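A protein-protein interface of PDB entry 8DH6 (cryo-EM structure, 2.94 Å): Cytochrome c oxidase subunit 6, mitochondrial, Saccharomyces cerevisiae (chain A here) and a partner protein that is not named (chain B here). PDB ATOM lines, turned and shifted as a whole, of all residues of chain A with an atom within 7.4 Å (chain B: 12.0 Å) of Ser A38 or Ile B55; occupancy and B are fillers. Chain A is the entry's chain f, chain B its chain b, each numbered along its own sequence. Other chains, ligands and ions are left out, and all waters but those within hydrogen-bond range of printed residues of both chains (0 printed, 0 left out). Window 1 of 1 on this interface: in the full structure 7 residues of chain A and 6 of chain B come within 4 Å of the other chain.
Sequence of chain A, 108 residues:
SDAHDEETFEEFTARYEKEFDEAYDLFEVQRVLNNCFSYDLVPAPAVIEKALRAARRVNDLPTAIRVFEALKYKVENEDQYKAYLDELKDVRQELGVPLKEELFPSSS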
ATOM      1  N   PHE A  12      -2.675 -18.092  -9.211  1.00  0.00           N
ATOM      2  CA  PHE A  12      -1.403 -18.794  -9.072  1.00  0.00           C
ATOM      3  C   PHE A  12      -1.455 -19.802  -7.931  1.00  0.00           C
ATOM      4  O   PHE A  12      -1.029 -20.955  -8.080  1.00  0.00           O
ATOM      5  CB  PHE A  12      -0.290 -17.770  -8.839  1.00  0.00           C
ATOM      6  CG  PHE A  12       1.056 -18.373  -8.569  1.00  0.00           C
ATOM      7  CD1 PHE A  12       1.926 -18.637  -9.606  1.00  0.00           C
ATOM      8  CD2 PHE A  12       1.457 -18.658  -7.276  1.00  0.00           C
ATOM      9  CE1 PHE A  12       3.164 -19.179  -9.361  1.00  0.00           C
ATOM     10  CE2 PHE A  12       2.691 -19.208  -7.027  1.00  0.00           C
ATOM     11  CZ  PHE A  12       3.548 -19.465  -8.071  1.00  0.00           C
ATOM     12  N   TYR A  16      -1.177 -23.892  -8.401  1.00  0.00           N
ATOM     13  CA  TYR A  16      -0.080 -24.691  -7.875  1.00  0.00           C
ATOM     14  C   TYR A  16      -0.505 -25.635  -6.757  1.00  0.00           C
ATOM     15  O   TYR A  16       0.107 -26.698  -6.615  1.00  0.00           O
ATOM     16  CB  TYR A  16       1.072 -23.794  -7.434  1.00  0.00           C
ATOM     17  CG  TYR A  16       2.061 -23.628  -8.557  1.00  0.00           C
ATOM     18  CD1 TYR A  16       2.948 -24.645  -8.872  1.00  0.00           C
ATOM     19  CD2 TYR A  16       2.076 -22.485  -9.337  1.00  0.00           C
ATOM     20  CE1 TYR A  16       3.838 -24.516  -9.913  1.00  0.00           C
ATOM     21  CE2 TYR A  16       2.967 -22.346 -10.379  1.00  0.00           C
ATOM     22  CZ  TYR A  16       3.847 -23.363 -10.661  1.00  0.00           C
ATOM     23  OH  TYR A  16       4.738 -23.231 -11.700  1.00  0.00           O
ATOM     24  N   ARG A  31       9.962 -30.868  -9.987  1.00  0.00           N
ATOM     25  CA  ARG A  31       9.722 -29.981 -11.123  1.00  0.00           C
ATOM     26  C   ARG A  31       8.668 -28.932 -10.794  1.00  0.00           C
ATOM     27  O   ARG A  31       8.826 -27.746 -11.121  1.00  0.00           O
ATOM     28  CB  ARG A  31       9.298 -30.802 -12.340  1.00  0.00           C
ATOM     29  CG  ARG A  31       8.866 -29.962 -13.523  1.00  0.00           C
ATOM     30  CD  ARG A  31       8.133 -30.789 -14.560  1.00  0.00           C
ATOM     31  NE  ARG A  31       6.835 -31.242 -14.080  1.00  0.00           N
ATOM     32  CZ  ARG A  31       5.734 -30.503 -14.091  1.00  0.00           C
ATOM     33  NH1 ARG A  31       5.744 -29.256 -14.526  1.00  0.00           N
ATOM     34  NH2 ARG A  31       4.596 -31.028 -13.648  1.00  0.00           N
ATOM     35  N   VAL A  32       7.574 -29.355 -10.159  1.00  0.00           N
ATOM     36  CA  VAL A  32       6.515 -28.424  -9.787  1.00  0.00           C
ATOM     37  C   VAL A  32       7.034 -27.408  -8.781  1.00  0.00           C
ATOM     38  O   VAL A  32       6.748 -26.212  -8.884  1.00  0.00           O
ATOM     39  CB  VAL A  32       5.297 -29.192  -9.247  1.00  0.00           C
ATOM     40  CG1 VAL A  32       4.325 -28.243  -8.583  1.00  0.00           C
ATOM     41  CG2 VAL A  32       4.614 -29.952 -10.364  1.00  0.00           C
ATOM     42  N   LEU A  33       7.819 -27.860  -7.801  1.00  0.00           N
ATOM     43  CA  LEU A  33       8.388 -26.934  -6.831  1.00  0.00           C
ATOM     44  C   LEU A  33       9.344 -25.952  -7.503  1.00  0.00           C
ATOM     45  O   LEU A  33       9.342 -24.755  -7.185  1.00  0.00           O
ATOM     46  CB  LEU A  33       9.087 -27.726  -5.729  1.00  0.00           C
ATOM     47  CG  LEU A  33       9.790 -26.988  -4.598  1.00  0.00           C
ATOM     48  CD1 LEU A  33       8.764 -26.323  -3.712  1.00  0.00           C
ATOM     49  CD2 LEU A  33      10.618 -27.972  -3.800  1.00  0.00           C
ATOM     50  N   ASN A  34      10.147 -26.437  -8.454  1.00  0.00           N
ATOM     51  CA  ASN A  34      11.094 -25.578  -9.156  1.00  0.00           C
ATOM     52  C   ASN A  34      10.380 -24.488  -9.938  1.00  0.00           C
ATOM     53  O   ASN A  34      10.689 -23.301  -9.787  1.00  0.00           O
ATOM     54  CB  ASN A  34      11.959 -26.412 -10.097  1.00  0.00           C
ATOM     55  CG  ASN A  34      13.133 -25.637 -10.643  1.00  0.00           C
ATOM     56  OD1 ASN A  34      13.663 -24.748  -9.979  1.00  0.00           O
ATOM     57  ND2 ASN A  34      13.549 -25.970 -11.856  1.00  0.00           N
ATOM     58  N   ASN A  35       9.419 -24.866 -10.775  1.00  0.00           N
ATOM     59  CA  ASN A  35       8.752 -23.854 -11.581  1.00  0.00           C
ATOM     60  C   ASN A  35       7.717 -23.067 -10.787  1.00  0.00           C
ATOM     61  O   ASN A  35       7.209 -22.062 -11.288  1.00  0.00           O
ATOM     62  CB  ASN A  35       8.137 -24.480 -12.842  1.00  0.00           C
ATOM     63  CG  ASN A  35       7.043 -25.483 -12.548  1.00  0.00           C
ATOM     64  OD1 ASN A  35       6.574 -25.607 -11.423  1.00  0.00           O
ATOM     65  ND2 ASN A  35       6.633 -26.213 -13.577  1.00  0.00           N
ATOM     66  N   CYS A  36       7.403 -23.492  -9.562  1.00  0.00           N
ATOM     67  CA  CYS A  36       6.666 -22.653  -8.628  1.00  0.00           C
ATOM     68  C   CYS A  36       7.543 -21.562  -8.036  1.00  0.00           C
ATOM     69  O   CYS A  36       7.099 -20.417  -7.900  1.00  0.00           O
ATOM     70  CB  CYS A  36       6.083 -23.507  -7.502  1.00  0.00           C
ATOM     71  SG  CYS A  36       5.161 -22.579  -6.268  1.00  0.00           S
ATOM     72  N   PHE A  37       8.783 -21.897  -7.680  1.00  0.00           N
ATOM     73  CA  PHE A  37       9.677 -20.921  -7.073  1.00  0.00           C
ATOM     74  C   PHE A  37      10.397 -20.050  -8.094  1.00  0.00           C
ATOM     75  O   PHE A  37      11.105 -19.122  -7.695  1.00  0.00           O
ATOM     76  CB  PHE A  37      10.701 -21.631  -6.187  1.00  0.00           C
ATOM     77  CG  PHE A  37      10.282 -21.737  -4.753  1.00  0.00           C
ATOM     78  CD1 PHE A  37      10.584 -20.732  -3.855  1.00  0.00           C
ATOM     79  CD2 PHE A  37       9.574 -22.836  -4.303  1.00  0.00           C
ATOM     80  CE1 PHE A  37      10.193 -20.825  -2.536  1.00  0.00           C
ATOM     81  CE2 PHE A  37       9.181 -22.932  -2.984  1.00  0.00           C
ATOM     82  CZ  PHE A  37       9.491 -21.927  -2.101  1.00  0.00           C
ATOM     83  N   SER A  38      10.239 -20.320  -9.389  1.00  0.00           N
ATOM     84  CA  SER A  38      10.900 -19.532 -10.430  1.00  0.00           C
ATOM     85  C   SER A  38       9.947 -18.456 -10.951  1.00  0.00           C
ATOM     86  O   SER A  38       9.670 -18.338 -12.145  1.00  0.00           O
ATOM     87  CB  SER A  38      11.383 -20.438 -11.554  1.00  0.00           C
ATOM     88  OG  SER A  38      12.349 -21.360 -11.083  1.00  0.00           O
ATOM     89  N   TYR A  39       9.456 -17.645 -10.018  1.00  0.00           N
ATOM     90  CA  TYR A  39       8.524 -16.570 -10.333  1.00  0.00           C
ATOM     91  C   TYR A  39       8.933 -15.329  -9.555  1.00  0.00           C
ATOM     92  O   TYR A  39       9.773 -15.384  -8.654  1.00  0.00           O
ATOM     93  CB  TYR A  39       7.082 -16.966 -10.008  1.00  0.00           C
ATOM     94  CG  TYR A  39       6.368 -17.693 -11.121  1.00  0.00           C
ATOM     95  CD1 TYR A  39       5.978 -17.029 -12.272  1.00  0.00           C
ATOM     96  CD2 TYR A  39       6.081 -19.043 -11.018  1.00  0.00           C
ATOM     97  CE1 TYR A  39       5.324 -17.690 -13.288  1.00  0.00           C
ATOM     98  CE2 TYR A  39       5.428 -19.711 -12.029  1.00  0.00           C
ATOM     99  CZ  TYR A  39       5.052 -19.032 -13.161  1.00  0.00           C
ATOM    100  OH  TYR A  39       4.402 -19.703 -14.168  1.00  0.00           O
ATOM    101  N   ASP A  40       8.325 -14.201  -9.905  1.00  0.00           N
ATOM    102  CA  ASP A  40       8.572 -12.948  -9.194  1.00  0.00           C
ATOM    103  C   ASP A  40       7.638 -12.787  -7.998  1.00  0.00           C
ATOM    104  O   ASP A  40       7.001 -11.753  -7.806  1.00  0.00           O
ATOM    105  CB  ASP A  40       8.455 -11.773 -10.162  1.00  0.00           C
ATOM    106  CG  ASP A  40       7.062 -11.632 -10.762  1.00  0.00           C
ATOM    107  OD1 ASP A  40       6.181 -12.468 -10.467  1.00  0.00           O
ATOM    108  OD2 ASP A  40       6.848 -10.676 -11.535  1.00  0.00           O
ATOM    109  N   LEU A  41       7.579 -13.826  -7.169  1.00  0.00           N
ATOM    110  CA  LEU A  41       6.716 -13.844  -5.998  1.00  0.00           C
ATOM    111  C   LEU A  41       7.067 -15.055  -5.149  1.00  0.00           C
ATOM    112  O   LEU A  41       7.433 -16.105  -5.682  1.00  0.00           O
ATOM    113  CB  LEU A  41       5.234 -13.880  -6.395  1.00  0.00           C
ATOM    114  CG  LEU A  41       4.731 -15.047  -7.248  1.00  0.00           C
ATOM    115  CD1 LEU A  41       4.213 -16.174  -6.376  1.00  0.00           C
ATOM    116  CD2 LEU A  41       3.650 -14.585  -8.209  1.00  0.00           C
ATOM    117  N   PRO A  43       5.769 -18.082  -2.973  1.00  0.00           N
ATOM    118  CA  PRO A  43       4.497 -18.809  -2.916  1.00  0.00           C
ATOM    119  C   PRO A  43       3.823 -18.677  -1.561  1.00  0.00           C
ATOM    120  O   PRO A  43       4.472 -18.544  -0.522  1.00  0.00           O
ATOM    121  CB  PRO A  43       4.907 -20.262  -3.187  1.00  0.00           C
ATOM    122  CG  PRO A  43       6.209 -20.163  -3.894  1.00  0.00           C
ATOM    123  CD  PRO A  43       6.892 -18.959  -3.341  1.00  0.00           C
ATOM    124  N   ALA A  70      14.673 -22.900   0.023  1.00  0.00           N
ATOM    125  CA  ALA A  70      14.329 -22.043  -1.103  1.00  0.00           C
ATOM    126  C   ALA A  70      13.465 -20.871  -0.670  1.00  0.00           C
ATOM    127  O   ALA A  70      13.610 -19.768  -1.206  1.00  0.00           O
ATOM    128  CB  ALA A  70      13.614 -22.856  -2.180  1.00  0.00           C
ATOM    129  N   TYR A  73      15.864 -18.427   0.795  1.00  0.00           N
ATOM    130  CA  TYR A  73      16.659 -17.794  -0.251  1.00  0.00           C
ATOM    131  C   TYR A  73      15.822 -16.948  -1.201  1.00  0.00           C
ATOM    132  O   TYR A  73      16.391 -16.217  -2.017  1.00  0.00           O
ATOM    133  CB  TYR A  73      17.418 -18.855  -1.052  1.00  0.00           C
ATOM    134  CG  TYR A  73      18.761 -19.230  -0.466  1.00  0.00           C
ATOM    135  CD1 TYR A  73      18.853 -19.842   0.777  1.00  0.00           C
ATOM    136  CD2 TYR A  73      19.937 -18.969  -1.154  1.00  0.00           C
ATOM    137  CE1 TYR A  73      20.078 -20.186   1.315  1.00  0.00           C
ATOM    138  CE2 TYR A  73      21.165 -19.310  -0.625  1.00  0.00           C
ATOM    139  CZ  TYR A  73      21.232 -19.918   0.609  1.00  0.00           C
ATOM    140  OH  TYR A  73      22.454 -20.257   1.140  1.00  0.00           O
ATOM    141  N   LYS A  74      14.495 -17.036  -1.116  1.00  0.00           N
ATOM    142  CA  LYS A  74      13.585 -16.337  -2.015  1.00  0.00           C
ATOM    143  C   LYS A  74      12.970 -15.100  -1.376  1.00  0.00           C
ATOM    144  O   LYS A  74      12.757 -14.091  -2.056  1.00  0.00           O
ATOM    145  CB  LYS A  74      12.469 -17.286  -2.461  1.00  0.00           C
ATOM    146  CG  LYS A  74      11.542 -16.725  -3.519  1.00  0.00           C
ATOM    147  CD  LYS A  74      12.249 -16.569  -4.847  1.00  0.00           C
ATOM    148  CE  LYS A  74      11.252 -16.361  -5.964  1.00  0.00           C
ATOM    149  NZ  LYS A  74      11.808 -16.789  -7.273  1.00  0.00           N
ATOM    150  N   ILE B  46      24.277  -6.477 -11.787  1.00  0.00           N
ATOM    151  CA  ILE B  46      23.643  -7.723 -12.196  1.00  0.00           C
ATOM    152  C   ILE B  46      24.584  -8.897 -11.970  1.00  0.00           C
ATOM    153  O   ILE B  46      24.188  -9.928 -11.414  1.00  0.00           O
ATOM    154  CB  ILE B  46      23.182  -7.640 -13.660  1.00  0.00           C
ATOM    155  CG1 ILE B  46      22.001  -6.680 -13.798  1.00  0.00           C
ATOM    156  CG2 ILE B  46      22.777  -8.996 -14.152  1.00  0.00           C
ATOM    157  CD1 ILE B  46      21.644  -6.369 -15.231  1.00  0.00           C
ATOM    158  N   VAL B  47      25.847  -8.759 -12.380  1.00  0.00           N
ATOM    159  CA  VAL B  47      26.780  -9.866 -12.209  1.00  0.00           C
ATOM    160  C   VAL B  47      26.983 -10.173 -10.733  1.00  0.00           C
ATOM    161  O   VAL B  47      26.815 -11.320 -10.304  1.00  0.00           O
ATOM    162  CB  VAL B  47      28.110  -9.568 -12.920  1.00  0.00           C
ATOM    163  CG1 VAL B  47      29.164 -10.577 -12.511  1.00  0.00           C
ATOM    164  CG2 VAL B  47      27.914  -9.603 -14.418  1.00  0.00           C
ATOM    165  N   THR B  49      25.109  -9.532  -8.230  1.00  0.00           N
ATOM    166  CA  THR B  49      23.920  -9.925  -7.489  1.00  0.00           C
ATOM    167  C   THR B  49      23.426 -11.306  -7.891  1.00  0.00           C
ATOM    168  O   THR B  49      22.999 -12.083  -7.031  1.00  0.00           O
ATOM    169  CB  THR B  49      22.806  -8.892  -7.689  1.00  0.00           C
ATOM    170  OG1 THR B  49      23.255  -7.611  -7.232  1.00  0.00           O
ATOM    171  CG2 THR B  49      21.564  -9.285  -6.909  1.00  0.00           C
ATOM    172  N   TYR B  50      23.490 -11.637  -9.180  1.00  0.00           N
ATOM    173  CA  TYR B  50      22.924 -12.873  -9.697  1.00  0.00           C
ATOM    174  C   TYR B  50      23.973 -13.938  -9.981  1.00  0.00           C
ATOM    175  O   TYR B  50      23.627 -15.010 -10.487  1.00  0.00           O
ATOM    176  CB  TYR B  50      22.100 -12.569 -10.947  1.00  0.00           C
ATOM    177  CG  TYR B  50      21.002 -11.569 -10.674  1.00  0.00           C
ATOM    178  CD1 TYR B  50      19.905 -11.910  -9.897  1.00  0.00           C
ATOM    179  CD2 TYR B  50      21.078 -10.274 -11.162  1.00  0.00           C
ATOM    180  CE1 TYR B  50      18.904 -10.998  -9.633  1.00  0.00           C
ATOM    181  CE2 TYR B  50      20.085  -9.355 -10.900  1.00  0.00           C
ATOM    182  CZ  TYR B  50      19.001  -9.722 -10.137  1.00  0.00           C
ATOM    183  OH  TYR B  50      18.009  -8.809  -9.874  1.00  0.00           O
ATOM    184  N   SER B  51      25.244 -13.685  -9.662  1.00  0.00           N
ATOM    185  CA  SER B  51      26.216 -14.766  -9.632  1.00  0.00           C
ATOM    186  C   SER B  51      26.070 -15.629  -8.390  1.00  0.00           C
ATOM    187  O   SER B  51      26.711 -16.681  -8.302  1.00  0.00           O
ATOM    188  CB  SER B  51      27.633 -14.200  -9.708  1.00  0.00           C
ATOM    189  OG  SER B  51      27.958 -13.485  -8.530  1.00  0.00           O
ATOM    190  N   LYS B  52      25.250 -15.199  -7.435  1.00  0.00           N
ATOM    191  CA  LYS B  52      24.958 -15.941  -6.217  1.00  0.00           C
ATOM    192  C   LYS B  52      23.453 -16.102  -6.026  1.00  0.00           C
ATOM    193  O   LYS B  52      22.960 -16.170  -4.900  1.00  0.00           O
ATOM    194  CB  LYS B  52      25.605 -15.256  -5.016  1.00  0.00           C
ATOM    195  CG  LYS B  52      25.047 -13.880  -4.705  1.00  0.00           C
ATOM    196  CD  LYS B  52      25.775 -13.251  -3.533  1.00  0.00           C
ATOM    197  CE  LYS B  52      25.207 -11.879  -3.206  1.00  0.00           C
ATOM    198  NZ  LYS B  52      25.912 -11.240  -2.064  1.00  0.00           N
ATOM    199  N   ASN B  53      22.715 -16.163  -7.136  1.00  0.00           N
ATOM    200  CA  ASN B  53      21.274 -16.363  -7.113  1.00  0.00           C
ATOM    201  C   ASN B  53      20.973 -17.825  -7.385  1.00  0.00           C
ATOM    202  O   ASN B  53      21.321 -18.323  -8.466  1.00  0.00           O
ATOM    203  CB  ASN B  53      20.599 -15.483  -8.159  1.00  0.00           C
ATOM    204  CG  ASN B  53      19.090 -15.489  -8.045  1.00  0.00           C
ATOM    205  OD1 ASN B  53      18.520 -16.171  -7.197  1.00  0.00           O
ATOM    206  ND2 ASN B  53      18.432 -14.727  -8.908  1.00  0.00           N
ATOM    207  N   PRO B  54      20.352 -18.549  -6.460  1.00  0.00           N
ATOM    208  CA  PRO B  54      20.088 -19.973  -6.698  1.00  0.00           C
ATOM    209  C   PRO B  54      18.926 -20.217  -7.647  1.00  0.00           C
ATOM    210  O   PRO B  54      18.919 -21.208  -8.383  1.00  0.00           O
ATOM    211  CB  PRO B  54      19.783 -20.505  -5.294  1.00  0.00           C
ATOM    212  CG  PRO B  54      19.230 -19.333  -4.574  1.00  0.00           C
ATOM    213  CD  PRO B  54      19.954 -18.131  -5.105  1.00  0.00           C
ATOM    214  N   ILE B  55      17.943 -19.322  -7.643  1.00  0.00           N
ATOM    215  CA  ILE B  55      16.714 -19.485  -8.412  1.00  0.00           C
ATOM    216  C   ILE B  55      16.705 -18.448  -9.524  1.00  0.00           C
ATOM    217  O   ILE B  55      16.766 -17.241  -9.260  1.00  0.00           O
ATOM    218  CB  ILE B  55      15.469 -19.348  -7.522  1.00  0.00           C
ATOM    219  CG1 ILE B  55      15.245 -20.628  -6.720  1.00  0.00           C
ATOM    220  CG2 ILE B  55      14.251 -19.035  -8.365  1.00  0.00           C
ATOM    221  CD1 ILE B  55      14.885 -21.816  -7.574  1.00  0.00           C
ATOM    222  N   ALA B  56      16.615 -18.915 -10.766  1.00  0.00           N
ATOM    223  CA  ALA B  56      16.608 -18.034 -11.925  1.00  0.00           C
ATOM    224  C   ALA B  56      15.175 -17.741 -12.345  1.00  0.00           C
ATOM    225  O   ALA B  56      14.371 -18.663 -12.518  1.00  0.00           O
ATOM    226  CB  ALA B  56      17.380 -18.663 -13.083  1.00  0.00           C
ATOM    227  N   TYR B  57      14.860 -16.458 -12.512  1.00  0.00           N
ATOM    228  CA  TYR B  57      13.537 -16.030 -12.964  1.00  0.00           C
ATOM    229  C   TYR B  57      13.424 -16.330 -14.455  1.00  0.00           C
ATOM    230  O   TYR B  57      13.543 -15.456 -15.316  1.00  0.00           O
ATOM    231  CB  TYR B  57      13.322 -14.553 -12.668  1.00  0.00           C
ATOM    232  CG  TYR B  57      13.479 -14.190 -11.212  1.00  0.00           C
ATOM    233  CD1 TYR B  57      12.532 -14.573 -10.275  1.00  0.00           C
ATOM    234  CD2 TYR B  57      14.581 -13.475 -10.772  1.00  0.00           C
ATOM    235  CE1 TYR B  57      12.673 -14.242  -8.945  1.00  0.00           C
ATOM    236  CE2 TYR B  57      14.729 -13.143  -9.441  1.00  0.00           C
ATOM    237  CZ  TYR B  57      13.774 -13.530  -8.532  1.00  0.00           C
ATOM    238  OH  TYR B  57      13.919 -13.200  -7.205  1.00  0.00           O
ATOM    239  N   LYS B  58      13.175 -17.601 -14.758  1.00  0.00           N
ATOM    240  CA  LYS B  58      13.176 -18.098 -16.127  1.00  0.00           C
ATOM    241  C   LYS B  58      11.881 -17.813 -16.873  1.00  0.00           C
ATOM    242  O   LYS B  58      11.708 -18.315 -17.988  1.00  0.00           O
ATOM    243  CB  LYS B  58      13.450 -19.603 -16.131  1.00  0.00           C
ATOM    244  CG  LYS B  58      12.487 -20.401 -15.275  1.00  0.00           C
ATOM    245  CD  LYS B  58      12.793 -21.885 -15.332  1.00  0.00           C
ATOM    246  CE  LYS B  58      11.695 -22.699 -14.675  1.00  0.00           C
ATOM    247  NZ  LYS B  58      11.838 -24.151 -14.962  1.00  0.00           N
ATOM    248  N   TYR B  59      10.969 -17.030 -16.298  1.00  0.00           N
ATOM    249  CA  TYR B  59       9.690 -16.743 -16.933  1.00  0.00           C
ATOM    250  C   TYR B  59       9.533 -15.276 -17.310  1.00  0.00           C
ATOM    251  O   TYR B  59       8.413 -14.840 -17.600  1.00  0.00           O
ATOM    252  CB  TYR B  59       8.539 -17.178 -16.023  1.00  0.00           C
ATOM    253  CG  TYR B  59       8.406 -18.676 -15.902  1.00  0.00           C
ATOM    254  CD1 TYR B  59       8.590 -19.497 -17.004  1.00  0.00           C
ATOM    255  CD2 TYR B  59       8.103 -19.271 -14.688  1.00  0.00           C
ATOM    256  CE1 TYR B  59       8.473 -20.863 -16.901  1.00  0.00           C
ATOM    257  CE2 TYR B  59       7.983 -20.639 -14.577  1.00  0.00           C
ATOM    258  CZ  TYR B  59       8.170 -21.429 -15.687  1.00  0.00           C
ATOM    259  OH  TYR B  59       8.054 -22.794 -15.588  1.00  0.00           O
ATOM    260  N   ILE B  60      10.616 -14.504 -17.307  1.00  0.00           N
ATOM    261  CA  ILE B  60      10.581 -13.102 -17.711  1.00  0.00           C
ATOM    262  C   ILE B  60      11.223 -13.029 -19.094  1.00  0.00           C
ATOM    263  O   ILE B  60      12.441 -13.138 -19.232  1.00  0.00           O
ATOM    264  CB  ILE B  60      11.296 -12.205 -16.701  1.00  0.00           C
ATOM    265  CG1 ILE B  60      10.585 -12.260 -15.349  1.00  0.00           C
ATOM    266  CG2 ILE B  60      11.341 -10.777 -17.204  1.00  0.00           C
ATOM    267  CD1 ILE B  60      11.359 -11.614 -14.227  1.00  0.00           C
ATOM    268  N   LYS B  61      10.397 -12.859 -20.126  1.00  0.00           N
ATOM    269  CA  LYS B  61      10.881 -12.917 -21.502  1.00  0.00           C
ATOM    270  C   LYS B  61      10.644 -11.628 -22.280  1.00  0.00           C
ATOM    271  O   LYS B  61      11.590 -11.100 -22.873  1.00  0.00           O
ATOM    272  CB  LYS B  61      10.242 -14.112 -22.218  1.00  0.00           C
ATOM    273  CG  LYS B  61      10.732 -15.455 -21.699  1.00  0.00           C
ATOM    274  CD  LYS B  61      10.177 -16.613 -22.510  1.00  0.00           C
ATOM    275  CE  LYS B  61       8.724 -16.878 -22.168  1.00  0.00           C
ATOM    276  NZ  LYS B  61       8.201 -18.085 -22.867  1.00  0.00           N
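The side-chain amide oxygen (OD1) of Asn B53 sits close to the backbone carbonyl oxygen (O) of Ile B55 (2.9 Å). The backbone carbonyl oxygen of Arg A31 lies close to the side-chain amide oxygen of Asn A35, at 3.1 Å. The side-chain amide oxygen of Asn A35 sits close to the backbone carbonyl oxygen of Val A32 (2.6 Å). The backbone carbonyl oxygen (O) of Asn A34 sits at hydrogen-bond distance from the side-chain hydroxyl (OG) of Ser A38, at 2.9 Å. The backbone carbonyl oxygen of Phe A37 lies within hydrogen-bond range of the side-chain amino group of Lys A74, 2.5 Å away. The backbone carbonyl oxygen of Tyr A39 is in hydrogen-bond range of the side-chain amino group of Lys A74, at 2.8 Å.
CD1 of Ile B55 touches OD1 of Asn A34, at 3.98 Å. Asn A35 touches Tyr B59. Ile B55 touches Phe A37. Ser A38 touches Ile B55. Ser A38 touches Ala B56 (CB to O, 3.6 Å). CB of Ser A38 touches CE of Lys B58, 3.9 Å away. O of Ser A38 touches CD2 of Tyr B59 (3.1 Å). Tyr B57 touches Tyr A39. Tyr A39 touches Tyr B59. Pro B54 touches Tyr A73.
Ser A38 touches just these residues of chain B: Ile B55 (3.97 Å), Ala B56 (3.6 Å), Lys B58 (3.9 Å) and Tyr B59 (3.1 Å). Of the printed residues of chain A, Ile B55 touches Asn A34 (3.98 Å), Phe A37 (3.2 Å), Ser A38 (3.97 Å) and Lys A74 (3.5 Å). Asn A35 touches just one residue of chain B: Tyr B59. Of chain B, only Ile B55 (3.2 Å) comes within 4 Å of Phe A37. Printed residues of chain A within 4 Å of Lys B58: Asn A34 (3.99 Å) and Ser A38 (3.9 Å). Of the printed residues of chain A, Pro B54 touches Tyr A73 (3.5 Å). Val A32 touches none of the printed residues of chain B. The nearest printed residue of chain A that does not touch Pro B54 is Lys A74 (6.3 Å).
Printed residues of chain A that touch a printed residue of chain B: Asn A34, Asn A35, Phe A37, Ser A38, Tyr A39, Tyr A73 and Lys A74. Of the 15 printed residues of chain B, 6 touch a printed residue of chain A. Hydrophobic or aromatic side chains of chain B that line the printed part of chain A: Pro B54, Ile B55, Tyr B57 and Tyr B59. Among the printed residues, no Asp or Glu carboxylate lies within 4 Å of a Lys or Arg side-chain nitrogen of the other chain.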
